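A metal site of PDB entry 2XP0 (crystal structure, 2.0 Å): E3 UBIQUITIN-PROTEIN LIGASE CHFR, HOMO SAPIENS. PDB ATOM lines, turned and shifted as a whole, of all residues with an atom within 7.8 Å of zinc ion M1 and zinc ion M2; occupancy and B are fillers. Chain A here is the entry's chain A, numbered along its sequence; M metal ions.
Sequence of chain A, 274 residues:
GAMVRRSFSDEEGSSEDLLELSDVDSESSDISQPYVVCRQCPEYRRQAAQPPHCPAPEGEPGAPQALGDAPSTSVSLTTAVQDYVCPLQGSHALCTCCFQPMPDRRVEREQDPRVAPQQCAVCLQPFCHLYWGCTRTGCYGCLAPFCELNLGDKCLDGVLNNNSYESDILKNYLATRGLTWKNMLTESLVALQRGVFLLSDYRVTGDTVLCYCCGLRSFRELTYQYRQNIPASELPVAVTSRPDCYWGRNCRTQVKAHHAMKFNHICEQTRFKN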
ATOM      1  N   ARG A  39      23.019 -18.696  -4.222  1.00  0.00           N
ATOM      2  CA  ARG A  39      21.740 -18.750  -4.937  1.00  0.00           C
ATOM      3  C   ARG A  39      21.264 -17.402  -5.481  1.00  0.00           C
ATOM      4  O   ARG A  39      20.618 -17.337  -6.516  1.00  0.00           O
ATOM      5  CB  ARG A  39      20.639 -19.318  -4.026  1.00  0.00           C
ATOM      6  CG  ARG A  39      20.556 -20.832  -3.955  1.00  0.00           C
ATOM      7  CD  ARG A  39      19.324 -21.266  -3.178  1.00  0.00           C
ATOM      8  NE  ARG A  39      19.655 -22.163  -2.075  1.00  0.00           N
ATOM      9  CZ  ARG A  39      18.766 -22.611  -1.186  1.00  0.00           C
ATOM     10  NH1 ARG A  39      17.494 -22.221  -1.272  1.00  0.00           N
ATOM     11  NH2 ARG A  39      19.138 -23.431  -0.213  1.00  0.00           N
ATOM     12  N   LEU A  94      28.028 -18.476   5.862  1.00  0.00           N
ATOM     13  CA  LEU A  94      27.764 -19.866   5.572  1.00  0.00           C
ATOM     14  C   LEU A  94      26.753 -20.444   6.547  1.00  0.00           C
ATOM     15  O   LEU A  94      26.867 -20.254   7.760  1.00  0.00           O
ATOM     16  CB  LEU A  94      29.062 -20.668   5.611  1.00  0.00           C
ATOM     17  CG  LEU A  94      30.156 -20.165   4.673  1.00  0.00           C
ATOM     18  CD1 LEU A  94      31.377 -21.084   4.744  1.00  0.00           C
ATOM     19  CD2 LEU A  94      29.646 -20.084   3.257  1.00  0.00           C
ATOM     20  N   CYS A  95      25.752 -21.129   6.013  1.00  0.00           N
ATOM     21  CA  CYS A  95      24.808 -21.849   6.866  1.00  0.00           C
ATOM     22  C   CYS A  95      25.553 -22.894   7.682  1.00  0.00           C
ATOM     23  O   CYS A  95      26.259 -23.736   7.135  1.00  0.00           O
ATOM     24  CB  CYS A  95      23.716 -22.502   6.031  1.00  0.00           C
ATOM     25  SG  CYS A  95      22.594 -23.528   7.031  1.00  0.00           S
ATOM     26  N   THR A  96      25.373 -22.823   8.999  1.00  0.00           N
ATOM     27  CA  THR A  96      25.996 -23.761   9.926  1.00  0.00           C
ATOM     28  C   THR A  96      25.577 -25.222   9.667  1.00  0.00           C
ATOM     29  O   THR A  96      26.310 -26.149  10.000  1.00  0.00           O
ATOM     30  CB  THR A  96      25.607 -23.352  11.369  1.00  0.00           C
ATOM     31  OG1 THR A  96      25.979 -21.982  11.585  1.00  0.00           O
ATOM     32  CG2 THR A  96      26.268 -24.260  12.386  1.00  0.00           C
ATOM     33  N   CYS A  97      24.404 -25.404   9.058  1.00  0.00           N
ATOM     34  CA  CYS A  97      23.886 -26.741   8.765  1.00  0.00           C
ATOM     35  C   CYS A  97      24.384 -27.322   7.437  1.00  0.00           C
ATOM     36  O   CYS A  97      24.946 -28.425   7.407  1.00  0.00           O
ATOM     37  CB  CYS A  97      22.345 -26.729   8.758  1.00  0.00           C
ATOM     38  SG  CYS A  97      21.610 -28.290   8.163  1.00  0.00           S
ATOM     39  N   CYS A  98      24.186 -26.600   6.339  1.00  0.00           N
ATOM     40  CA  CYS A  98      24.491 -27.172   5.033  1.00  0.00           C
ATOM     41  C   CYS A  98      25.795 -26.635   4.427  1.00  0.00           C
ATOM     42  O   CYS A  98      26.215 -27.073   3.361  1.00  0.00           O
ATOM     43  CB  CYS A  98      23.337 -26.914   4.067  1.00  0.00           C
ATOM     44  SG  CYS A  98      23.178 -25.180   3.662  1.00  0.00           S
ATOM     45  N   PHE A  99      26.421 -25.670   5.107  1.00  0.00           N
ATOM     46  CA  PHE A  99      27.702 -25.091   4.676  1.00  0.00           C
ATOM     47  C   PHE A  99      27.627 -24.255   3.400  1.00  0.00           C
ATOM     48  O   PHE A  99      28.647 -23.834   2.863  1.00  0.00           O
ATOM     49  CB  PHE A  99      28.775 -26.188   4.514  1.00  0.00           C
ATOM     50  CG  PHE A  99      28.834 -27.160   5.655  1.00  0.00           C
ATOM     51  CD1 PHE A  99      29.094 -26.719   6.949  1.00  0.00           C
ATOM     52  CD2 PHE A  99      28.636 -28.515   5.437  1.00  0.00           C
ATOM     53  CE1 PHE A  99      29.150 -27.615   8.001  1.00  0.00           C
ATOM     54  CE2 PHE A  99      28.683 -29.417   6.493  1.00  0.00           C
ATOM     55  CZ  PHE A  99      28.946 -28.962   7.783  1.00  0.00           C
ATOM     56  N   GLN A 100      26.413 -23.994   2.918  1.00  0.00           N
ATOM     57  CA  GLN A 100      26.250 -23.198   1.702  1.00  0.00           C
ATOM     58  C   GLN A 100      26.132 -21.726   2.055  1.00  0.00           C
ATOM     59  O   GLN A 100      25.525 -21.374   3.068  1.00  0.00           O
ATOM     60  CB  GLN A 100      25.020 -23.651   0.922  1.00  0.00           C
ATOM     61  CG  GLN A 100      25.011 -25.130   0.612  1.00  0.00           C
ATOM     62  CD  GLN A 100      26.225 -25.571  -0.159  1.00  0.00           C
ATOM     63  OE1 GLN A 100      26.373 -25.240  -1.331  1.00  0.00           O
ATOM     64  NE2 GLN A 100      27.115 -26.310   0.487  1.00  0.00           N
ATOM     65  N   PRO A 101      26.701 -20.862   1.218  1.00  0.00           N
ATOM     66  CA  PRO A 101      26.640 -19.409   1.425  1.00  0.00           C
ATOM     67  C   PRO A 101      25.244 -18.846   1.186  1.00  0.00           C
ATOM     68  O   PRO A 101      24.529 -19.301   0.306  1.00  0.00           O
ATOM     69  CB  PRO A 101      27.578 -18.871   0.349  1.00  0.00           C
ATOM     70  CG  PRO A 101      27.545 -19.913  -0.717  1.00  0.00           C
ATOM     71  CD  PRO A 101      27.520 -21.197   0.037  1.00  0.00           C
ATOM     72  N   MET A 102      24.882 -17.867   2.001  1.00  0.00           N
ATOM     73  CA  MET A 102      23.682 -17.074   1.773  1.00  0.00           C
ATOM     74  C   MET A 102      24.095 -15.628   2.027  1.00  0.00           C
ATOM     75  O   MET A 102      25.086 -15.367   2.704  1.00  0.00           O
ATOM     76  CB  MET A 102      22.590 -17.478   2.753  1.00  0.00           C
ATOM     77  CG  MET A 102      22.955 -17.234   4.209  1.00  0.00           C
ATOM     78  SD  MET A 102      21.726 -17.806   5.403  1.00  0.00           S
ATOM     79  CE  MET A 102      22.634 -17.537   6.915  1.00  0.00           C
ATOM     80  N   PRO A 126      24.610 -18.795  12.243  1.00  0.00           N
ATOM     81  CA  PRO A 126      23.738 -18.596  11.076  1.00  0.00           C
ATOM     82  C   PRO A 126      23.170 -19.908  10.517  1.00  0.00           C
ATOM     83  O   PRO A 126      23.880 -20.908  10.462  1.00  0.00           O
ATOM     84  CB  PRO A 126      24.689 -17.951  10.048  1.00  0.00           C
ATOM     85  CG  PRO A 126      26.034 -18.456  10.413  1.00  0.00           C
ATOM     86  CD  PRO A 126      26.037 -18.590  11.928  1.00  0.00           C
ATOM     87  N   PHE A 127      21.908 -19.875  10.094  1.00  0.00           N
ATOM     88  CA  PHE A 127      21.282 -21.007   9.407  1.00  0.00           C
ATOM     89  C   PHE A 127      20.394 -20.460   8.308  1.00  0.00           C
ATOM     90  O   PHE A 127      19.802 -19.403   8.480  1.00  0.00           O
ATOM     91  CB  PHE A 127      20.419 -21.837  10.368  1.00  0.00           C
ATOM     92  CG  PHE A 127      21.196 -22.551  11.423  1.00  0.00           C
ATOM     93  CD1 PHE A 127      21.613 -23.862  11.218  1.00  0.00           C
ATOM     94  CD2 PHE A 127      21.504 -21.933  12.605  1.00  0.00           C
ATOM     95  CE1 PHE A 127      22.328 -24.538  12.196  1.00  0.00           C
ATOM     96  CE2 PHE A 127      22.225 -22.582  13.576  1.00  0.00           C
ATOM     97  CZ  PHE A 127      22.641 -23.893  13.372  1.00  0.00           C
ATOM     98  N   CYS A 128      20.286 -21.185   7.194  1.00  0.00           N
ATOM     99  CA  CYS A 128      19.621 -20.632   6.010  1.00  0.00           C
ATOM    100  C   CYS A 128      18.143 -21.015   5.850  1.00  0.00           C
ATOM    101  O   CYS A 128      17.479 -20.528   4.931  1.00  0.00           O
ATOM    102  CB  CYS A 128      20.372 -21.040   4.723  1.00  0.00           C
ATOM    103  SG  CYS A 128      20.072 -22.741   4.150  1.00  0.00           S
ATOM    104  N   HIS A 129      17.620 -21.871   6.726  1.00  0.00           N
ATOM    105  CA  HIS A 129      16.325 -22.479   6.423  1.00  0.00           C
ATOM    106  C   HIS A 129      15.147 -21.513   6.280  1.00  0.00           C
ATOM    107  O   HIS A 129      14.400 -21.603   5.311  1.00  0.00           O
ATOM    108  CB  HIS A 129      15.970 -23.578   7.425  1.00  0.00           C
ATOM    109  CG  HIS A 129      14.799 -24.411   6.982  1.00  0.00           C
ATOM    110  ND1 HIS A 129      14.813 -25.145   5.821  1.00  0.00           N
ATOM    111  CD2 HIS A 129      13.592 -24.639   7.564  1.00  0.00           C
ATOM    112  CE1 HIS A 129      13.659 -25.795   5.702  1.00  0.00           C
ATOM    113  NE2 HIS A 129      12.909 -25.496   6.739  1.00  0.00           N
ATOM    114  N   LEU A 130      14.960 -20.627   7.252  1.00  0.00           N
ATOM    115  CA  LEU A 130      13.829 -19.710   7.191  1.00  0.00           C
ATOM    116  C   LEU A 130      14.027 -18.718   6.049  1.00  0.00           C
ATOM    117  O   LEU A 130      13.051 -18.267   5.462  1.00  0.00           O
ATOM    118  CB  LEU A 130      13.652 -18.974   8.516  1.00  0.00           C
ATOM    119  CG  LEU A 130      13.109 -19.890   9.609  1.00  0.00           C
ATOM    120  CD1 LEU A 130      13.052 -19.185  10.944  1.00  0.00           C
ATOM    121  CD2 LEU A 130      11.733 -20.401   9.210  1.00  0.00           C
ATOM    122  N   TRP A 132      15.606 -19.172   2.974  1.00  0.00           N
ATOM    123  CA  TRP A 132      15.297 -19.682   1.633  1.00  0.00           C
ATOM    124  C   TRP A 132      15.160 -21.196   1.485  1.00  0.00           C
ATOM    125  O   TRP A 132      15.079 -21.703   0.373  1.00  0.00           O
ATOM    126  CB  TRP A 132      16.298 -19.126   0.591  1.00  0.00           C
ATOM    127  CG  TRP A 132      17.742 -19.568   0.762  1.00  0.00           C
ATOM    128  CD1 TRP A 132      18.205 -20.617   1.499  1.00  0.00           C
ATOM    129  CD2 TRP A 132      18.894 -18.962   0.156  1.00  0.00           C
ATOM    130  NE1 TRP A 132      19.576 -20.695   1.402  1.00  0.00           N
ATOM    131  CE2 TRP A 132      20.021 -19.694   0.587  1.00  0.00           C
ATOM    132  CE3 TRP A 132      19.095 -17.856  -0.685  1.00  0.00           C
ATOM    133  CZ2 TRP A 132      21.319 -19.363   0.193  1.00  0.00           C
ATOM    134  CZ3 TRP A 132      20.376 -17.535  -1.074  1.00  0.00           C
ATOM    135  CH2 TRP A 132      21.478 -18.282  -0.634  1.00  0.00           C
ATOM    136  N   GLY A 133      15.124 -21.922   2.608  1.00  0.00           N
ATOM    137  CA  GLY A 133      14.942 -23.363   2.561  1.00  0.00           C
ATOM    138  C   GLY A 133      16.278 -24.066   2.466  1.00  0.00           C
ATOM    139  O   GLY A 133      17.000 -23.907   1.477  1.00  0.00           O
ATOM    140  N   CYS A 134      16.621 -24.831   3.486  1.00  0.00           N
ATOM    141  CA  CYS A 134      17.884 -25.549   3.537  1.00  0.00           C
ATOM    142  C   CYS A 134      17.639 -26.993   3.107  1.00  0.00           C
ATOM    143  O   CYS A 134      16.609 -27.562   3.436  1.00  0.00           O
ATOM    144  CB  CYS A 134      18.425 -25.525   4.977  1.00  0.00           C
ATOM    145  SG  CYS A 134      20.015 -26.391   5.243  1.00  0.00           S
ATOM    146  N   THR A 135      18.570 -27.586   2.382  1.00  0.00           N
ATOM    147  CA  THR A 135      18.454 -29.005   2.012  1.00  0.00           C
ATOM    148  C   THR A 135      19.732 -29.781   2.312  1.00  0.00           C
ATOM    149  O   THR A 135      20.816 -29.435   1.828  1.00  0.00           O
ATOM    150  CB  THR A 135      18.115 -29.188   0.526  1.00  0.00           C
ATOM    151  OG1 THR A 135      16.847 -28.594   0.251  1.00  0.00           O
ATOM    152  CG2 THR A 135      18.046 -30.671   0.178  1.00  0.00           C
ATOM    153  N   ARG A 136      19.600 -30.846   3.108  1.00  0.00           N
ATOM    154  CA  ARG A 136      20.710 -31.740   3.388  1.00  0.00           C
ATOM    155  C   ARG A 136      20.162 -32.980   4.056  1.00  0.00           C
ATOM    156  O   ARG A 136      19.262 -32.893   4.899  1.00  0.00           O
ATOM    157  CB  ARG A 136      21.741 -31.072   4.317  1.00  0.00           C
ATOM    158  CG  ARG A 136      22.916 -31.979   4.690  1.00  0.00           C
ATOM    159  CD  ARG A 136      23.952 -31.310   5.597  1.00  0.00           C
ATOM    160  NE  ARG A 136      23.408 -30.983   6.914  1.00  0.00           N
ATOM    161  CZ  ARG A 136      23.267 -31.852   7.913  1.00  0.00           C
ATOM    162  NH1 ARG A 136      23.621 -33.129   7.759  1.00  0.00           N
ATOM    163  NH2 ARG A 136      22.758 -31.454   9.072  1.00  0.00           N
ATOM    164  N   GLY A 138      19.828 -35.398   6.730  1.00  0.00           N
ATOM    165  CA  GLY A 138      20.080 -35.180   8.135  1.00  0.00           C
ATOM    166  C   GLY A 138      19.494 -33.854   8.575  1.00  0.00           C
ATOM    167  O   GLY A 138      19.301 -33.633   9.769  1.00  0.00           O
ATOM    168  N   CYS A 139      19.215 -32.974   7.620  1.00  0.00           N
ATOM    169  CA  CYS A 139      18.526 -31.722   7.921  1.00  0.00           C
ATOM    170  C   CYS A 139      17.015 -31.896   7.852  1.00  0.00           C
ATOM    171  O   CYS A 139      16.460 -32.247   6.808  1.00  0.00           O
ATOM    172  CB  CYS A 139      18.974 -30.584   7.005  1.00  0.00           C
ATOM    173  SG  CYS A 139      18.051 -29.043   7.280  1.00  0.00           S
ATOM    174  N   TYR A 140      16.367 -31.645   8.989  1.00  0.00           N
ATOM    175  CA  TYR A 140      14.927 -31.774   9.124  1.00  0.00           C
ATOM    176  C   TYR A 140      14.200 -30.462   8.845  1.00  0.00           C
ATOM    177  O   TYR A 140      12.961 -30.428   8.794  1.00  0.00           O
ATOM    178  CB  TYR A 140      14.586 -32.200  10.550  1.00  0.00           C
ATOM    179  CG  TYR A 140      15.254 -33.481  10.993  1.00  0.00           C
ATOM    180  CD1 TYR A 140      15.222 -34.624  10.200  1.00  0.00           C
ATOM    181  CD2 TYR A 140      15.885 -33.567  12.225  1.00  0.00           C
ATOM    182  CE1 TYR A 140      15.814 -35.801  10.607  1.00  0.00           C
ATOM    183  CE2 TYR A 140      16.491 -34.734  12.649  1.00  0.00           C
ATOM    184  CZ  TYR A 140      16.456 -35.845  11.838  1.00  0.00           C
ATOM    185  OH  TYR A 140      17.038 -37.015  12.258  1.00  0.00           O
ATOM    186  N   GLY A 141      14.969 -29.385   8.683  1.00  0.00           N
ATOM    187  CA  GLY A 141      14.449 -28.026   8.786  1.00  0.00           C
ATOM    188  C   GLY A 141      15.122 -27.344   9.965  1.00  0.00           C
ATOM    189  O   GLY A 141      14.573 -27.292  11.078  1.00  0.00           O
ATOM    190  N   CYS A 142      16.316 -26.797   9.717  1.00  0.00           N
ATOM    191  CA  CYS A 142      17.266 -26.480  10.780  1.00  0.00           C
ATOM    192  C   CYS A 142      17.034 -25.183  11.573  1.00  0.00           C
ATOM    193  O   CYS A 142      17.772 -24.912  12.516  1.00  0.00           O
ATOM    194  CB  CYS A 142      18.693 -26.478  10.224  1.00  0.00           C
ATOM    195  SG  CYS A 142      18.911 -25.446   8.765  1.00  0.00           S
ATOM    196  N   LEU A 143      16.033 -24.404  11.196  1.00  0.00           N
ATOM    197  CA  LEU A 143      15.720 -23.174  11.927  1.00  0.00           C
ATOM    198  C   LEU A 143      14.207 -22.964  11.956  1.00  0.00           C
ATOM    199  O   LEU A 143      13.562 -23.041  10.919  1.00  0.00           O
ATOM    200  CB  LEU A 143      16.441 -21.953  11.296  1.00  0.00           C
ATOM    201  CG  LEU A 143      16.481 -20.639  12.094  1.00  0.00           C
ATOM    202  CD1 LEU A 143      17.333 -20.810  13.354  1.00  0.00           C
ATOM    203  CD2 LEU A 143      16.973 -19.445  11.260  1.00  0.00           C
ATOM    204  N   TYR A 212      18.178 -26.628  15.197  1.00  0.00           N
ATOM    205  CA  TYR A 212      17.983 -28.030  15.553  1.00  0.00           C
ATOM    206  C   TYR A 212      18.675 -28.417  16.854  1.00  0.00           C
ATOM    207  O   TYR A 212      18.042 -28.951  17.763  1.00  0.00           O
ATOM    208  CB  TYR A 212      18.502 -28.930  14.423  1.00  0.00           C
ATOM    209  CG  TYR A 212      18.566 -30.378  14.844  1.00  0.00           C
ATOM    210  CD1 TYR A 212      17.411 -31.132  14.988  1.00  0.00           C
ATOM    211  CD2 TYR A 212      19.792 -30.987  15.111  1.00  0.00           C
ATOM    212  CE1 TYR A 212      17.469 -32.468  15.376  1.00  0.00           C
ATOM    213  CE2 TYR A 212      19.861 -32.305  15.493  1.00  0.00           C
ATOM    214  CZ  TYR A 212      18.703 -33.037  15.634  1.00  0.00           C
ATOM    215  OH  TYR A 212      18.788 -34.356  16.023  1.00  0.00           O
HETATM  216 ZN    ZN M   1      21.401 -24.379   5.109  1.00  0.00          ZN
HETATM  217 ZN    ZN M   2      19.678 -27.304   7.387  1.00  0.00          ZN
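The side-chain sulfur (SG) of Cys 95 lies close to the backbone NH (N) of Cys 97 (3.3 Å). The backbone carbonyl oxygen of Cys 97 sits at hydrogen-bond distance from the guanidinium group of Arg 136, at 3.0 Å. SG of Cys 139 sits close to N of Gly 141, at 3.4 Å. N of Cys 95 is in hydrogen-bond range of O of Gln 100. O of Cys 142 lies within hydrogen-bond range of N of Tyr 212, 3.2 Å away. A ring nitrogen (ND1) of His 129 lies within hydrogen-bond range of the backbone NH of Cys 134 (3.0 Å). SG of Cys 128 lies close to NE1 of Trp 132. O of Cys 98 sits at hydrogen-bond distance from NE2 of Gln 100, at 3.1 Å.
Four residues have an atom within 4 Å of zinc ion M1: Cys 95, Cys 98, Cys 128 and Cys 134. The nearest printed residue that does not touch zinc ion M1 is Cys 97 (4.4 Å).
Of the 27 residues printed, 4 come within 4 Å of zinc ion M2. Along chain A the residues within 4 Å of zinc ion M2 span positions 97 to 142.
Zinc ion M1 is bound by SG of Cys 128 (2.3 Å), SG of Cys 95 (2.4 Å), SG of Cys 98 (2.4 Å) and SG of Cys 134 (2.4 Å).
Zinc ion M2 is bound by the side-chain sulfur (SG) of Cys 97 (2.3 Å), the side-chain sulfur (SG) of Cys 134 (2.4 Å), the side-chain sulfur (SG) of Cys 139 (2.4 Å) and the side-chain sulfur (SG) of Cys 142 (2.4 Å).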
